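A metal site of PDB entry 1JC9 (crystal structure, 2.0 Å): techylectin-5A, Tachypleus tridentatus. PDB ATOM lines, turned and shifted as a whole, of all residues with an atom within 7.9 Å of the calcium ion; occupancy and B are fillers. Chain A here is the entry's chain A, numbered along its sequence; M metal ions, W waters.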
ATOM      1  N   SER A 193      -1.008 -23.469  -0.018  1.00  0.00           N
ATOM      2  CA  SER A 193      -0.042 -24.038  -0.950  1.00  0.00           C
ATOM      3  C   SER A 193       0.492 -25.368  -0.443  1.00  0.00           C
ATOM      4  O   SER A 193       0.525 -25.607   0.769  1.00  0.00           O
ATOM      5  CB  SER A 193       1.150 -23.090  -1.178  1.00  0.00           C
ATOM      6  OG  SER A 193       0.771 -21.922  -1.879  1.00  0.00           O
ATOM      7  N   LYS A 197       1.584 -27.680  -5.476  1.00  0.00           N
ATOM      8  CA  LYS A 197       0.796 -26.557  -5.957  1.00  0.00           C
ATOM      9  C   LYS A 197       1.202 -25.236  -5.327  1.00  0.00           C
ATOM     10  O   LYS A 197       0.844 -24.940  -4.184  1.00  0.00           O
ATOM     11  CB  LYS A 197      -0.701 -26.808  -5.737  1.00  0.00           C
ATOM     12  CG  LYS A 197      -1.235 -27.955  -6.571  1.00  0.00           C
ATOM     13  CD  LYS A 197      -2.752 -28.029  -6.529  1.00  0.00           C
ATOM     14  CE  LYS A 197      -3.262 -29.131  -7.442  1.00  0.00           C
ATOM     15  NZ  LYS A 197      -4.752 -29.257  -7.384  1.00  0.00           N
ATOM     16  N   ASP A 198       1.938 -24.435  -6.093  1.00  0.00           N
ATOM     17  CA  ASP A 198       2.437 -23.124  -5.668  1.00  0.00           C
ATOM     18  C   ASP A 198       1.393 -22.026  -5.869  1.00  0.00           C
ATOM     19  O   ASP A 198       1.151 -21.600  -7.002  1.00  0.00           O
ATOM     20  CB  ASP A 198       3.698 -22.759  -6.446  1.00  0.00           C
ATOM     21  CG  ASP A 198       4.341 -21.468  -5.968  1.00  0.00           C
ATOM     22  OD1 ASP A 198       3.623 -20.580  -5.469  1.00  0.00           O
ATOM     23  OD2 ASP A 198       5.578 -21.341  -6.085  1.00  0.00           O
ATOM     24  N   HIS A 199       0.789 -21.571  -4.780  1.00  0.00           N
ATOM     25  CA  HIS A 199      -0.206 -20.510  -4.841  1.00  0.00           C
ATOM     26  C   HIS A 199       0.223 -19.302  -4.011  1.00  0.00           C
ATOM     27  O   HIS A 199      -0.582 -18.411  -3.744  1.00  0.00           O
ATOM     28  CB  HIS A 199      -1.548 -21.033  -4.329  1.00  0.00           C
ATOM     29  CG  HIS A 199      -2.126 -22.146  -5.146  1.00  0.00           C
ATOM     30  ND1 HIS A 199      -2.728 -23.247  -4.585  1.00  0.00           N
ATOM     31  CD2 HIS A 199      -2.223 -22.315  -6.492  1.00  0.00           C
ATOM     32  CE1 HIS A 199      -3.155 -24.053  -5.541  1.00  0.00           C
ATOM     33  NE2 HIS A 199      -2.861 -23.509  -6.708  1.00  0.00           N
ATOM     34  N   ASP A 200       1.494 -19.273  -3.605  1.00  0.00           N
ATOM     35  CA  ASP A 200       1.980 -18.166  -2.786  1.00  0.00           C
ATOM     36  C   ASP A 200       2.304 -16.924  -3.619  1.00  0.00           C
ATOM     37  O   ASP A 200       2.094 -16.899  -4.830  1.00  0.00           O
ATOM     38  CB  ASP A 200       3.194 -18.621  -1.966  1.00  0.00           C
ATOM     39  CG  ASP A 200       4.387 -18.991  -2.835  1.00  0.00           C
ATOM     40  OD1 ASP A 200       4.943 -20.090  -2.640  1.00  0.00           O
ATOM     41  OD2 ASP A 200       4.778 -18.176  -3.706  1.00  0.00           O
ATOM     42  N   THR A 201       2.811 -15.885  -2.964  1.00  0.00           N
ATOM     43  CA  THR A 201       3.139 -14.644  -3.654  1.00  0.00           C
ATOM     44  C   THR A 201       4.640 -14.398  -3.703  1.00  0.00           C
ATOM     45  O   THR A 201       5.099 -13.253  -3.643  1.00  0.00           O
ATOM     46  CB  THR A 201       2.478 -13.434  -2.969  1.00  0.00           C
ATOM     47  OG1 THR A 201       3.019 -13.281  -1.650  1.00  0.00           O
ATOM     48  CG2 THR A 201       0.976 -13.625  -2.899  1.00  0.00           C
ATOM     49  N   HIS A 202       5.408 -15.479  -3.810  1.00  0.00           N
ATOM     50  CA  HIS A 202       6.853 -15.375  -3.858  1.00  0.00           C
ATOM     51  C   HIS A 202       7.349 -15.978  -5.171  1.00  0.00           C
ATOM     52  O   HIS A 202       6.673 -16.799  -5.790  1.00  0.00           O
ATOM     53  CB  HIS A 202       7.454 -16.118  -2.666  1.00  0.00           C
ATOM     54  CG  HIS A 202       8.922 -15.857  -2.457  1.00  0.00           C
ATOM     55  ND1 HIS A 202       9.888 -16.373  -3.283  1.00  0.00           N
ATOM     56  CD2 HIS A 202       9.567 -15.138  -1.510  1.00  0.00           C
ATOM     57  CE1 HIS A 202      11.077 -15.987  -2.855  1.00  0.00           C
ATOM     58  NE2 HIS A 202      10.916 -15.236  -1.781  1.00  0.00           N
ATOM     59  N   GLU A 203       8.532 -15.540  -5.601  1.00  0.00           N
ATOM     60  CA  GLU A 203       9.124 -16.035  -6.839  1.00  0.00           C
ATOM     61  C   GLU A 203       9.416 -17.528  -6.726  1.00  0.00           C
ATOM     62  O   GLU A 203       9.315 -18.275  -7.690  1.00  0.00           O
ATOM     63  CB  GLU A 203      10.438 -15.285  -7.137  1.00  0.00           C
ATOM     64  CG  GLU A 203      10.281 -13.782  -7.285  1.00  0.00           C
ATOM     65  CD  GLU A 203       9.753 -13.116  -6.037  1.00  0.00           C
ATOM     66  OE1 GLU A 203      10.367 -13.281  -4.955  1.00  0.00           O
ATOM     67  OE2 GLU A 203       8.713 -12.421  -6.119  1.00  0.00           O
ATOM     68  N   THR A 204       9.792 -17.950  -5.516  1.00  0.00           N
ATOM     69  CA  THR A 204      10.109 -19.349  -5.277  1.00  0.00           C
ATOM     70  C   THR A 204       8.871 -20.157  -4.876  1.00  0.00           C
ATOM     71  O   THR A 204       7.760 -19.638  -4.833  1.00  0.00           O
ATOM     72  CB  THR A 204      11.148 -19.495  -4.153  1.00  0.00           C
ATOM     73  OG1 THR A 204      10.604 -19.002  -2.928  1.00  0.00           O
ATOM     74  CG2 THR A 204      12.396 -18.701  -4.499  1.00  0.00           C
ATOM     75  N   HIS A 205       9.096 -21.432  -4.581  1.00  0.00           N
ATOM     76  CA  HIS A 205       8.050 -22.361  -4.173  1.00  0.00           C
ATOM     77  C   HIS A 205       8.190 -22.499  -2.651  1.00  0.00           C
ATOM     78  O   HIS A 205       8.947 -23.330  -2.149  1.00  0.00           O
ATOM     79  CB  HIS A 205       8.295 -23.721  -4.845  1.00  0.00           C
ATOM     80  CG  HIS A 205       7.089 -24.607  -4.888  1.00  0.00           C
ATOM     81  ND1 HIS A 205       6.187 -24.695  -3.845  1.00  0.00           N
ATOM     82  CD2 HIS A 205       6.663 -25.485  -5.832  1.00  0.00           C
ATOM     83  CE1 HIS A 205       5.263 -25.586  -4.148  1.00  0.00           C
ATOM     84  NE2 HIS A 205       5.532 -26.079  -5.342  1.00  0.00           N
ATOM     85  N   CYS A 206       7.463 -21.653  -1.923  1.00  0.00           N
ATOM     86  CA  CYS A 206       7.519 -21.663  -0.466  1.00  0.00           C
ATOM     87  C   CYS A 206       7.319 -23.049   0.168  1.00  0.00           C
ATOM     88  O   CYS A 206       8.057 -23.430   1.062  1.00  0.00           O
ATOM     89  CB  CYS A 206       6.465 -20.712   0.112  1.00  0.00           C
ATOM     90  SG  CYS A 206       6.756 -18.925  -0.138  1.00  0.00           S
ATOM     91  N   ALA A 207       6.324 -23.780  -0.310  1.00  0.00           N
ATOM     92  CA  ALA A 207       6.018 -25.103   0.220  1.00  0.00           C
ATOM     93  C   ALA A 207       7.159 -26.110   0.073  1.00  0.00           C
ATOM     94  O   ALA A 207       7.383 -26.931   0.969  1.00  0.00           O
ATOM     95  CB  ALA A 207       4.750 -25.662  -0.440  1.00  0.00           C
ATOM     96  N   ASP A 217       3.021 -16.972   2.320  1.00  0.00           N
ATOM     97  CA  ASP A 217       3.085 -15.616   1.784  1.00  0.00           C
ATOM     98  C   ASP A 217       4.414 -15.437   1.063  1.00  0.00           C
ATOM     99  O   ASP A 217       4.526 -15.748  -0.128  1.00  0.00           O
ATOM    100  CB  ASP A 217       2.975 -14.590   2.918  1.00  0.00           C
ATOM    101  CG  ASP A 217       2.984 -13.162   2.417  1.00  0.00           C
ATOM    102  OD1 ASP A 217       3.028 -12.237   3.266  1.00  0.00           O
ATOM    103  OD2 ASP A 217       2.943 -12.950   1.180  1.00  0.00           O
ATOM    104  N   CYS A 219       7.937 -16.004   3.006  1.00  0.00           N
ATOM    105  CA  CYS A 219       7.006 -17.105   2.897  1.00  0.00           C
ATOM    106  C   CYS A 219       6.143 -17.294   4.150  1.00  0.00           C
ATOM    107  O   CYS A 219       4.944 -17.573   4.050  1.00  0.00           O
ATOM    108  CB  CYS A 219       7.763 -18.399   2.633  1.00  0.00           C
ATOM    109  SG  CYS A 219       8.435 -18.583   0.953  1.00  0.00           S
HETATM  110 CA    CA M   1       5.695 -19.078  -5.689  1.00  0.00          CA
HETATM  111  O   HOH W   1       6.595 -19.089  -8.129  1.00  0.00           O
HETATM  112  O   HOH W   2       3.959 -17.872  -6.605  1.00  0.00           O
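The backbone NH (N) of Thr 204 sits at hydrogen-bond distance from a ring nitrogen (ND1) of His 202, at 2.7 Å.
OD1 of Asp 200 is in hydrogen-bond range of N of Cys 206.
N of Asp 200 lies within hydrogen-bond range of OG of Ser 193 (3.2 Å).
SG of Cys 206 is disulfide-bonded to SG of Cys 219, 2.0 Å away.
Of the 14 residues printed, 4 come within 4 Å of the calcium ion.
The nearest printed residue that does not touch the calcium ion is Glu 203 (4.2 Å).
The calcium ion is bound by the side-chain carboxylate (OD2) of Asp 198 (2.3 Å), water W2 (2.3 Å), the backbone carbonyl oxygen (O) of Thr 204 (2.3 Å), the side-chain carboxylate (OD2) of Asp 200 (2.4 Å), the backbone carbonyl oxygen (O) of His 202 (2.5 Å), the side-chain carboxylate (OD1) of Asp 198 (2.6 Å) and water W1 (2.6 Å).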
